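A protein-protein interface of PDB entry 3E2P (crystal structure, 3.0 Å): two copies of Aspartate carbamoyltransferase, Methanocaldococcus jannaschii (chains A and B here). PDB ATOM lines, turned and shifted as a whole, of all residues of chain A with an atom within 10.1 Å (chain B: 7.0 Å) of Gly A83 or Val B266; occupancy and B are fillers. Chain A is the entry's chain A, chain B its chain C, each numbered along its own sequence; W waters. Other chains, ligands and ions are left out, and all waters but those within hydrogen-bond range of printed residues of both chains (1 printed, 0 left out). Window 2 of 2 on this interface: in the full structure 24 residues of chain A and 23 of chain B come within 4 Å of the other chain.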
ATOM      1  N   TYR A  48     -19.278  -6.626  -0.219  1.00  0.00           N
ATOM      2  CA  TYR A  48     -20.716  -6.431  -0.100  1.00  0.00           C
ATOM      3  C   TYR A  48     -21.314  -7.805   0.175  1.00  0.00           C
ATOM      4  O   TYR A  48     -22.131  -7.971   1.089  1.00  0.00           O
ATOM      5  CB  TYR A  48     -21.282  -5.808  -1.368  1.00  0.00           C
ATOM      6  CG  TYR A  48     -21.025  -4.315  -1.433  1.00  0.00           C
ATOM      7  CD1 TYR A  48     -19.756  -3.807  -1.726  1.00  0.00           C
ATOM      8  CD2 TYR A  48     -22.047  -3.411  -1.168  1.00  0.00           C
ATOM      9  CE1 TYR A  48     -19.517  -2.432  -1.754  1.00  0.00           C
ATOM     10  CE2 TYR A  48     -21.822  -2.038  -1.191  1.00  0.00           C
ATOM     11  CZ  TYR A  48     -20.559  -1.549  -1.484  1.00  0.00           C
ATOM     12  OH  TYR A  48     -20.363  -0.177  -1.511  1.00  0.00           O
ATOM     13  N   LEU A  75     -21.532  -5.114   3.685  1.00  0.00           N
ATOM     14  CA  LEU A  75     -21.929  -3.787   3.228  1.00  0.00           C
ATOM     15  C   LEU A  75     -23.340  -3.848   2.670  1.00  0.00           C
ATOM     16  O   LEU A  75     -24.009  -2.825   2.506  1.00  0.00           O
ATOM     17  CB  LEU A  75     -20.987  -3.300   2.128  1.00  0.00           C
ATOM     18  CG  LEU A  75     -19.938  -2.264   2.532  1.00  0.00           C
ATOM     19  CD1 LEU A  75     -19.056  -1.953   1.347  1.00  0.00           C
ATOM     20  CD2 LEU A  75     -20.620  -1.001   3.034  1.00  0.00           C
ATOM     21  N   LYS A  76     -23.776  -5.069   2.375  1.00  0.00           N
ATOM     22  CA  LYS A  76     -25.092  -5.303   1.810  1.00  0.00           C
ATOM     23  C   LYS A  76     -26.230  -4.907   2.741  1.00  0.00           C
ATOM     24  O   LYS A  76     -27.234  -4.361   2.292  1.00  0.00           O
ATOM     25  CB  LYS A  76     -25.230  -6.773   1.406  1.00  0.00           C
ATOM     26  CG  LYS A  76     -26.422  -7.045   0.505  1.00  0.00           C
ATOM     27  CD  LYS A  76     -26.500  -6.030  -0.639  1.00  0.00           C
ATOM     28  CE  LYS A  76     -25.243  -6.027  -1.495  1.00  0.00           C
ATOM     29  NZ  LYS A  76     -25.264  -4.913  -2.484  1.00  0.00           N
ATOM     30  N   SER A  77     -26.085  -5.179   4.032  1.00  0.00           N
ATOM     31  CA  SER A  77     -27.135  -4.813   4.975  1.00  0.00           C
ATOM     32  C   SER A  77     -27.251  -3.293   4.987  1.00  0.00           C
ATOM     33  O   SER A  77     -26.272  -2.585   4.750  1.00  0.00           O
ATOM     34  CB  SER A  77     -26.822  -5.335   6.389  1.00  0.00           C
ATOM     35  OG  SER A  77     -25.728  -4.655   6.981  1.00  0.00           O
ATOM     36  N   SER A  78     -28.456  -2.799   5.245  1.00  0.00           N
ATOM     37  CA  SER A  78     -28.700  -1.365   5.284  1.00  0.00           C
ATOM     38  C   SER A  78     -28.013  -0.732   6.489  1.00  0.00           C
ATOM     39  O   SER A  78     -27.853   0.487   6.555  1.00  0.00           O
ATOM     40  CB  SER A  78     -30.204  -1.098   5.332  1.00  0.00           C
ATOM     41  OG  SER A  78     -30.815  -1.859   6.359  1.00  0.00           O
ATOM     42  N   SER A  79     -27.611  -1.566   7.442  1.00  0.00           N
ATOM     43  CA  SER A  79     -26.928  -1.081   8.634  1.00  0.00           C
ATOM     44  C   SER A  79     -25.467  -0.775   8.306  1.00  0.00           C
ATOM     45  O   SER A  79     -24.880   0.152   8.869  1.00  0.00           O
ATOM     46  CB  SER A  79     -27.002  -2.121   9.765  1.00  0.00           C
ATOM     47  OG  SER A  79     -28.323  -2.272  10.265  1.00  0.00           O
ATOM     48  N   VAL A  80     -24.884  -1.550   7.389  1.00  0.00           N
ATOM     49  CA  VAL A  80     -23.489  -1.357   6.994  1.00  0.00           C
ATOM     50  C   VAL A  80     -23.380  -0.562   5.689  1.00  0.00           C
ATOM     51  O   VAL A  80     -22.277  -0.232   5.251  1.00  0.00           O
ATOM     52  CB  VAL A  80     -22.750  -2.719   6.822  1.00  0.00           C
ATOM     53  CG1 VAL A  80     -21.244  -2.496   6.657  1.00  0.00           C
ATOM     54  CG2 VAL A  80     -23.019  -3.614   8.022  1.00  0.00           C
ATOM     55  N   ALA A  81     -24.522  -0.250   5.076  1.00  0.00           N
ATOM     56  CA  ALA A  81     -24.546   0.517   3.825  1.00  0.00           C
ATOM     57  C   ALA A  81     -25.198   1.890   4.012  1.00  0.00           C
ATOM     58  O   ALA A  81     -24.583   2.919   3.740  1.00  0.00           O
ATOM     59  CB  ALA A  81     -25.282  -0.268   2.734  1.00  0.00           C
ATOM     60  N   LYS A  82     -26.449   1.890   4.467  1.00  0.00           N
ATOM     61  CA  LYS A  82     -27.204   3.119   4.713  1.00  0.00           C
ATOM     62  C   LYS A  82     -27.618   3.896   3.454  1.00  0.00           C
ATOM     63  O   LYS A  82     -27.681   5.127   3.468  1.00  0.00           O
ATOM     64  CB  LYS A  82     -26.421   4.030   5.672  1.00  0.00           C
ATOM     65  CG  LYS A  82     -26.198   3.421   7.060  1.00  0.00           C
ATOM     66  CD  LYS A  82     -25.415   4.347   7.991  1.00  0.00           C
ATOM     67  CE  LYS A  82     -26.178   5.633   8.296  1.00  0.00           C
ATOM     68  NZ  LYS A  82     -27.505   5.374   8.931  1.00  0.00           N
ATOM     69  N   GLY A  83     -27.901   3.170   2.374  1.00  0.00           N
ATOM     70  CA  GLY A  83     -28.340   3.786   1.129  1.00  0.00           C
ATOM     71  C   GLY A  83     -27.281   4.522   0.331  1.00  0.00           C
ATOM     72  O   GLY A  83     -27.590   5.185  -0.662  1.00  0.00           O
ATOM     73  N   GLU A  84     -26.030   4.403   0.768  1.00  0.00           N
ATOM     74  CA  GLU A  84     -24.902   5.050   0.108  1.00  0.00           C
ATOM     75  C   GLU A  84     -24.466   4.193  -1.073  1.00  0.00           C
ATOM     76  O   GLU A  84     -24.378   2.976  -0.956  1.00  0.00           O
ATOM     77  CB  GLU A  84     -23.747   5.219   1.099  1.00  0.00           C
ATOM     78  CG  GLU A  84     -22.519   5.881   0.520  1.00  0.00           C
ATOM     79  CD  GLU A  84     -21.460   6.159   1.560  1.00  0.00           C
ATOM     80  OE1 GLU A  84     -20.956   5.198   2.188  1.00  0.00           O
ATOM     81  OE2 GLU A  84     -21.135   7.348   1.749  1.00  0.00           O
ATOM     82  N   SER A  85     -24.190   4.826  -2.207  1.00  0.00           N
ATOM     83  CA  SER A  85     -23.787   4.087  -3.396  1.00  0.00           C
ATOM     84  C   SER A  85     -22.355   3.580  -3.367  1.00  0.00           C
ATOM     85  O   SER A  85     -21.504   4.131  -2.674  1.00  0.00           O
ATOM     86  CB  SER A  85     -23.975   4.940  -4.650  1.00  0.00           C
ATOM     87  OG  SER A  85     -23.065   6.016  -4.665  1.00  0.00           O
ATOM     88  N   LEU A  86     -22.112   2.520  -4.135  1.00  0.00           N
ATOM     89  CA  LEU A  86     -20.793   1.923  -4.241  1.00  0.00           C
ATOM     90  C   LEU A  86     -19.806   3.032  -4.578  1.00  0.00           C
ATOM     91  O   LEU A  86     -18.729   3.141  -3.990  1.00  0.00           O
ATOM     92  CB  LEU A  86     -20.786   0.884  -5.362  1.00  0.00           C
ATOM     93  CG  LEU A  86     -19.432   0.272  -5.728  1.00  0.00           C
ATOM     94  CD1 LEU A  86     -18.895  -0.509  -4.547  1.00  0.00           C
ATOM     95  CD2 LEU A  86     -19.588  -0.632  -6.939  1.00  0.00           C
ATOM     96  N   ILE A  87     -20.194   3.861  -5.536  1.00  0.00           N
ATOM     97  CA  ILE A  87     -19.367   4.971  -5.970  1.00  0.00           C
ATOM     98  C   ILE A  87     -18.936   5.890  -4.829  1.00  0.00           C
ATOM     99  O   ILE A  87     -17.775   6.264  -4.740  1.00  0.00           O
ATOM    100  CB  ILE A  87     -20.092   5.768  -7.060  1.00  0.00           C
ATOM    101  CG1 ILE A  87     -19.750   5.166  -8.418  1.00  0.00           C
ATOM    102  CG2 ILE A  87     -19.701   7.225  -7.008  1.00  0.00           C
ATOM    103  CD1 ILE A  87     -20.332   5.929  -9.567  1.00  0.00           C
ATOM    104  N   ASP A  88     -19.861   6.254  -3.954  1.00  0.00           N
ATOM    105  CA  ASP A  88     -19.509   7.114  -2.835  1.00  0.00           C
ATOM    106  C   ASP A  88     -18.586   6.384  -1.870  1.00  0.00           C
ATOM    107  O   ASP A  88     -17.590   6.943  -1.416  1.00  0.00           O
ATOM    108  CB  ASP A  88     -20.762   7.578  -2.103  1.00  0.00           C
ATOM    109  CG  ASP A  88     -21.462   8.711  -2.818  1.00  0.00           C
ATOM    110  OD1 ASP A  88     -20.994   9.120  -3.904  1.00  0.00           O
ATOM    111  OD2 ASP A  88     -22.485   9.196  -2.288  1.00  0.00           O
ATOM    112  N   THR A  89     -18.916   5.133  -1.565  1.00  0.00           N
ATOM    113  CA  THR A  89     -18.106   4.336  -0.656  1.00  0.00           C
ATOM    114  C   THR A  89     -16.690   4.182  -1.189  1.00  0.00           C
ATOM    115  O   THR A  89     -15.733   4.410  -0.451  1.00  0.00           O
ATOM    116  CB  THR A  89     -18.701   2.932  -0.440  1.00  0.00           C
ATOM    117  OG1 THR A  89     -20.036   3.047   0.061  1.00  0.00           O
ATOM    118  CG2 THR A  89     -17.869   2.153   0.558  1.00  0.00           C
ATOM    119  N   ARG A  91     -15.073   6.065  -3.149  1.00  0.00           N
ATOM    120  CA  ARG A  91     -14.390   7.346  -3.029  1.00  0.00           C
ATOM    121  C   ARG A  91     -13.939   7.636  -1.600  1.00  0.00           C
ATOM    122  O   ARG A  91     -12.835   8.116  -1.386  1.00  0.00           O
ATOM    123  CB  ARG A  91     -15.266   8.474  -3.565  1.00  0.00           C
ATOM    124  CG  ARG A  91     -15.153   8.565  -5.071  1.00  0.00           C
ATOM    125  CD  ARG A  91     -15.910   9.729  -5.654  1.00  0.00           C
ATOM    126  NE  ARG A  91     -17.346   9.516  -5.580  1.00  0.00           N
ATOM    127  CZ  ARG A  91     -18.239  10.174  -6.311  1.00  0.00           C
ATOM    128  NH1 ARG A  91     -17.838  11.092  -7.178  1.00  0.00           N
ATOM    129  NH2 ARG A  91     -19.535   9.922  -6.168  1.00  0.00           N
ATOM    130  N   ARG B  53     -18.699   3.476   9.282  1.00  0.00           N
ATOM    131  CA  ARG B  53     -17.994   4.695   8.882  1.00  0.00           C
ATOM    132  C   ARG B  53     -17.092   5.266   9.971  1.00  0.00           C
ATOM    133  O   ARG B  53     -15.897   5.450   9.761  1.00  0.00           O
ATOM    134  CB  ARG B  53     -18.981   5.772   8.438  1.00  0.00           C
ATOM    135  CG  ARG B  53     -19.766   5.362   7.232  1.00  0.00           C
ATOM    136  CD  ARG B  53     -20.535   6.501   6.595  1.00  0.00           C
ATOM    137  NE  ARG B  53     -21.426   5.941   5.591  1.00  0.00           N
ATOM    138  CZ  ARG B  53     -22.381   5.059   5.873  1.00  0.00           C
ATOM    139  NH1 ARG B  53     -22.567   4.654   7.132  1.00  0.00           N
ATOM    140  NH2 ARG B  53     -23.127   4.558   4.897  1.00  0.00           N
ATOM    141  N   ARG B 226     -28.724  15.742   5.985  1.00  0.00           N
ATOM    142  CA  ARG B 226     -29.775  14.859   5.479  1.00  0.00           C
ATOM    143  C   ARG B 226     -31.156  15.204   6.021  1.00  0.00           C
ATOM    144  O   ARG B 226     -31.271  15.909   7.017  1.00  0.00           O
ATOM    145  CB  ARG B 226     -29.451  13.407   5.844  1.00  0.00           C
ATOM    146  CG  ARG B 226     -28.215  12.847   5.164  1.00  0.00           C
ATOM    147  CD  ARG B 226     -27.795  11.523   5.783  1.00  0.00           C
ATOM    148  NE  ARG B 226     -27.027  11.717   7.012  1.00  0.00           N
ATOM    149  CZ  ARG B 226     -26.712  10.746   7.865  1.00  0.00           C
ATOM    150  NH1 ARG B 226     -27.101   9.498   7.637  1.00  0.00           N
ATOM    151  NH2 ARG B 226     -25.995  11.023   8.946  1.00  0.00           N
ATOM    152  N   TYR B 238     -42.747  14.183   1.617  1.00  0.00           N
ATOM    153  CA  TYR B 238     -41.313  13.939   1.557  1.00  0.00           C
ATOM    154  C   TYR B 238     -40.731  14.253   0.180  1.00  0.00           C
ATOM    155  O   TYR B 238     -39.728  14.952   0.065  1.00  0.00           O
ATOM    156  CB  TYR B 238     -41.031  12.478   1.932  1.00  0.00           C
ATOM    157  CG  TYR B 238     -39.568  12.149   2.066  1.00  0.00           C
ATOM    158  CD1 TYR B 238     -38.786  12.750   3.050  1.00  0.00           C
ATOM    159  CD2 TYR B 238     -38.958  11.249   1.200  1.00  0.00           C
ATOM    160  CE1 TYR B 238     -37.424  12.461   3.165  1.00  0.00           C
ATOM    161  CE2 TYR B 238     -37.605  10.953   1.307  1.00  0.00           C
ATOM    162  CZ  TYR B 238     -36.847  11.562   2.288  1.00  0.00           C
ATOM    163  OH  TYR B 238     -35.515  11.264   2.389  1.00  0.00           O
ATOM    164  N   LYS B 242     -37.771  16.895  -0.550  1.00  0.00           N
ATOM    165  CA  LYS B 242     -36.512  16.488  -1.157  1.00  0.00           C
ATOM    166  C   LYS B 242     -36.178  17.393  -2.321  1.00  0.00           C
ATOM    167  O   LYS B 242     -35.082  17.928  -2.395  1.00  0.00           O
ATOM    168  CB  LYS B 242     -36.581  15.036  -1.644  1.00  0.00           C
ATOM    169  CG  LYS B 242     -36.418  13.987  -0.552  1.00  0.00           C
ATOM    170  CD  LYS B 242     -36.750  12.596  -1.068  1.00  0.00           C
ATOM    171  CE  LYS B 242     -35.813  12.138  -2.170  1.00  0.00           C
ATOM    172  NZ  LYS B 242     -36.205  10.789  -2.680  1.00  0.00           N
ATOM    173  N   LYS B 246     -32.885  19.935  -2.492  1.00  0.00           N
ATOM    174  CA  LYS B 246     -31.827  19.186  -3.134  1.00  0.00           C
ATOM    175  C   LYS B 246     -30.857  20.146  -3.780  1.00  0.00           C
ATOM    176  O   LYS B 246     -31.265  21.070  -4.469  1.00  0.00           O
ATOM    177  CB  LYS B 246     -32.397  18.242  -4.187  1.00  0.00           C
ATOM    178  CG  LYS B 246     -31.340  17.353  -4.802  1.00  0.00           C
ATOM    179  CD  LYS B 246     -31.952  16.228  -5.607  1.00  0.00           C
ATOM    180  CE  LYS B 246     -30.897  15.195  -5.964  1.00  0.00           C
ATOM    181  NZ  LYS B 246     -31.469  14.036  -6.699  1.00  0.00           N
ATOM    182  N   HIS B 261     -20.784  18.188   3.577  1.00  0.00           N
ATOM    183  CA  HIS B 261     -21.802  17.199   3.912  1.00  0.00           C
ATOM    184  C   HIS B 261     -21.105  16.107   4.697  1.00  0.00           C
ATOM    185  O   HIS B 261     -20.214  15.437   4.188  1.00  0.00           O
ATOM    186  CB  HIS B 261     -22.410  16.601   2.648  1.00  0.00           C
ATOM    187  CG  HIS B 261     -23.593  15.719   2.900  1.00  0.00           C
ATOM    188  ND1 HIS B 261     -23.586  14.712   3.839  1.00  0.00           N
ATOM    189  CD2 HIS B 261     -24.811  15.674   2.313  1.00  0.00           C
ATOM    190  CE1 HIS B 261     -24.748  14.085   3.818  1.00  0.00           C
ATOM    191  NE2 HIS B 261     -25.510  14.649   2.901  1.00  0.00           N
ATOM    192  N   PRO B 264     -23.280   9.884   5.173  1.00  0.00           N
ATOM    193  CA  PRO B 264     -23.385   9.599   3.742  1.00  0.00           C
ATOM    194  C   PRO B 264     -24.458  10.452   3.085  1.00  0.00           C
ATOM    195  O   PRO B 264     -25.470  10.779   3.710  1.00  0.00           O
ATOM    196  CB  PRO B 264     -23.758   8.123   3.724  1.00  0.00           C
ATOM    197  CG  PRO B 264     -24.685   8.026   4.900  1.00  0.00           C
ATOM    198  CD  PRO B 264     -23.936   8.822   5.962  1.00  0.00           C
ATOM    199  N   ARG B 265     -24.240  10.823   1.831  1.00  0.00           N
ATOM    200  CA  ARG B 265     -25.260  11.595   1.148  1.00  0.00           C
ATOM    201  C   ARG B 265     -26.059  10.624   0.309  1.00  0.00           C
ATOM    202  O   ARG B 265     -25.514   9.678  -0.259  1.00  0.00           O
ATOM    203  CB  ARG B 265     -24.652  12.685   0.271  1.00  0.00           C
ATOM    204  CG  ARG B 265     -23.932  12.195  -0.951  1.00  0.00           C
ATOM    205  CD  ARG B 265     -24.846  11.922  -2.122  1.00  0.00           C
ATOM    206  NE  ARG B 265     -24.019  11.503  -3.249  1.00  0.00           N
ATOM    207  CZ  ARG B 265     -23.274  12.324  -3.985  1.00  0.00           C
ATOM    208  NH1 ARG B 265     -23.258  13.627  -3.737  1.00  0.00           N
ATOM    209  NH2 ARG B 265     -22.496  11.834  -4.939  1.00  0.00           N
ATOM    210  N   VAL B 266     -27.359  10.865   0.245  1.00  0.00           N
ATOM    211  CA  VAL B 266     -28.255  10.004  -0.497  1.00  0.00           C
ATOM    212  C   VAL B 266     -29.044  10.822  -1.512  1.00  0.00           C
ATOM    213  O   VAL B 266     -28.932  10.600  -2.715  1.00  0.00           O
ATOM    214  CB  VAL B 266     -29.230   9.295   0.471  1.00  0.00           C
ATOM    215  CG1 VAL B 266     -29.855   8.095  -0.209  1.00  0.00           C
ATOM    216  CG2 VAL B 266     -28.500   8.878   1.731  1.00  0.00           C
ATOM    217  N   ASP B 267     -29.833  11.774  -1.025  1.00  0.00           N
ATOM    218  CA  ASP B 267     -30.635  12.615  -1.903  1.00  0.00           C
ATOM    219  C   ASP B 267     -30.207  14.080  -1.864  1.00  0.00           C
ATOM    220  O   ASP B 267     -30.331  14.802  -2.851  1.00  0.00           O
ATOM    221  CB  ASP B 267     -32.101  12.527  -1.500  1.00  0.00           C
ATOM    222  CG  ASP B 267     -32.593  11.108  -1.422  1.00  0.00           C
ATOM    223  OD1 ASP B 267     -32.485  10.391  -2.437  1.00  0.00           O
ATOM    224  OD2 ASP B 267     -33.086  10.713  -0.347  1.00  0.00           O
ATOM    225  N   GLU B 268     -29.700  14.503  -0.713  1.00  0.00           N
ATOM    226  CA  GLU B 268     -29.271  15.877  -0.478  1.00  0.00           C
ATOM    227  C   GLU B 268     -28.476  16.581  -1.584  1.00  0.00           C
ATOM    228  O   GLU B 268     -28.625  17.786  -1.779  1.00  0.00           O
ATOM    229  CB  GLU B 268     -28.471  15.941   0.832  1.00  0.00           C
ATOM    230  CG  GLU B 268     -29.071  15.146   1.989  1.00  0.00           C
ATOM    231  CD  GLU B 268     -28.809  13.659   1.869  1.00  0.00           C
ATOM    232  OE1 GLU B 268     -29.395  12.875   2.646  1.00  0.00           O
ATOM    233  OE2 GLU B 268     -28.011  13.270   0.999  1.00  0.00           O
ATOM    234  N   ILE B 269     -27.645  15.847  -2.308  1.00  0.00           N
ATOM    235  CA  ILE B 269     -26.823  16.454  -3.341  1.00  0.00           C
ATOM    236  C   ILE B 269     -26.761  15.609  -4.603  1.00  0.00           C
ATOM    237  O   ILE B 269     -26.436  14.422  -4.538  1.00  0.00           O
ATOM    238  CB  ILE B 269     -25.372  16.656  -2.818  1.00  0.00           C
ATOM    239  CG1 ILE B 269     -25.399  17.487  -1.526  1.00  0.00           C
ATOM    240  CG2 ILE B 269     -24.499  17.307  -3.893  1.00  0.00           C
ATOM    241  CD1 ILE B 269     -24.058  17.590  -0.822  1.00  0.00           C
ATOM    242  N   ASP B 270     -27.055  16.209  -5.754  1.00  0.00           N
ATOM    243  CA  ASP B 270     -27.005  15.471  -7.017  1.00  0.00           C
ATOM    244  C   ASP B 270     -25.607  14.980  -7.331  1.00  0.00           C
ATOM    245  O   ASP B 270     -24.625  15.603  -6.930  1.00  0.00           O
ATOM    246  CB  ASP B 270     -27.500  16.333  -8.168  1.00  0.00           C
ATOM    247  CG  ASP B 270     -28.936  16.055  -8.509  1.00  0.00           C
ATOM    248  OD1 ASP B 270     -29.274  14.864  -8.676  1.00  0.00           O
ATOM    249  OD2 ASP B 270     -29.723  17.017  -8.613  1.00  0.00           O
ATOM    250  N   TYR B 271     -25.515  13.869  -8.058  1.00  0.00           N
ATOM    251  CA  TYR B 271     -24.213  13.317  -8.397  1.00  0.00           C
ATOM    252  C   TYR B 271     -23.448  14.174  -9.384  1.00  0.00           C
ATOM    253  O   TYR B 271     -22.223  14.143  -9.404  1.00  0.00           O
ATOM    254  CB  TYR B 271     -24.345  11.888  -8.933  1.00  0.00           C
ATOM    255  CG  TYR B 271     -24.694  10.891  -7.857  1.00  0.00           C
ATOM    256  CD1 TYR B 271     -26.009  10.705  -7.454  1.00  0.00           C
ATOM    257  CD2 TYR B 271     -23.699  10.191  -7.185  1.00  0.00           C
ATOM    258  CE1 TYR B 271     -26.327   9.855  -6.406  1.00  0.00           C
ATOM    259  CE2 TYR B 271     -24.004   9.341  -6.136  1.00  0.00           C
ATOM    260  CZ  TYR B 271     -25.322   9.179  -5.748  1.00  0.00           C
ATOM    261  OH  TYR B 271     -25.633   8.367  -4.679  1.00  0.00           O
HETATM  262  O   HOH W   1     -24.504   7.537  -2.287  1.00  0.00           O
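Among the printed residues, pairs that only touch across the chains: Lys A82 with Arg B53 (3.0 Å), Gly A83 with Val B266 (3.7 Å), Glu A84 with Pro B264 (3.4 Å), Asp A88 with Tyr B271 (3.8 Å) and Arg A91 with Arg B265 (3.7 Å).
Of chain B, only Val B266 (3.7 Å) comes within 4 Å of Gly A83. Val B266 touches one residue of chain A. No residue of chain A comes within 4 Å of Asp B267. Of the printed residues of chain A, Tyr B271 touches Ser A85 (3.5 Å) and Asp A88 (3.8 Å). Of the printed residues of chain B, Lys A82 touches Arg B53. Leu A75 touches none of the printed residues of chain B. The nearest residue of chain B that does not touch Gly A83 is Arg B265 (5.0 Å).
The backbone carbonyl oxygen (O) of Ser A85 lies within hydrogen-bond range of the side-chain hydroxyl (OG1) of Thr A89, at 3.3 Å. The side-chain carboxylate (OD1) of Asp A88 is in salt-bridge range of the guanidinium group (NH2) of Arg A91 (2.8 Å). The side-chain hydroxyl (OG) of Ser A85 lies within hydrogen-bond range of the backbone NH (N) of Asp A88 (3.3 Å). OE2 of Glu B268 is in hydrogen-bond range of N of Val B266 (2.6 Å). The side-chain carboxylate (OE1) of Glu A84 sits at hydrogen-bond distance from the side-chain hydroxyl (OG1) of Thr A89 (3.2 Å). The backbone carbonyl oxygen (O) of Ile A87 is in hydrogen-bond range of the guanidinium group (NE) of Arg A91, 3.4 Å away.
Water W1 lies within hydrogen-bond range of OD2 of Asp A88 (2.6 Å), N of Ser A85 (2.7 Å), OH of Tyr B271 (2.8 Å) and O of Arg B265 (3.1 Å).
No position is printed for both chains. Of the 9 pairs that touch across the chains among the printed residues, none has its exchanged pair printed and touching as well.
Hydrophobic or aromatic side chains of chain B within 4 Å of the printed part of chain A: Pro B264, Val B266 and Tyr B271. Printed residues of chain A that touch a printed residue of chain B: Ala A81, Lys A82, Gly A83, Glu A84, Ser A85, Asp A88 and Arg A91. Among the printed residues, Asp or Glu carboxylates within 4 Å of a Lys or Arg side-chain nitrogen of the other chain: Glu A84 with Arg B53 (3.5 Å) and Asp A88 with Arg B265 (2.9 Å).
The guanidinium group (NE) of Arg B265 lies within salt-bridge range of the side-chain carboxylate (OD2) of Asp A88 (2.9 Å). The side-chain carboxylate of Glu A84 lies within salt-bridge range of the guanidinium group of Arg B53, at 3.5 Å. O of Ala A81 lies within hydrogen-bond range of NH2 of Arg B53, 2.5 Å away. The side-chain hydroxyl of Tyr B271 is in hydrogen-bond range of the side-chain hydroxyl of Ser A85 (3.5 Å).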
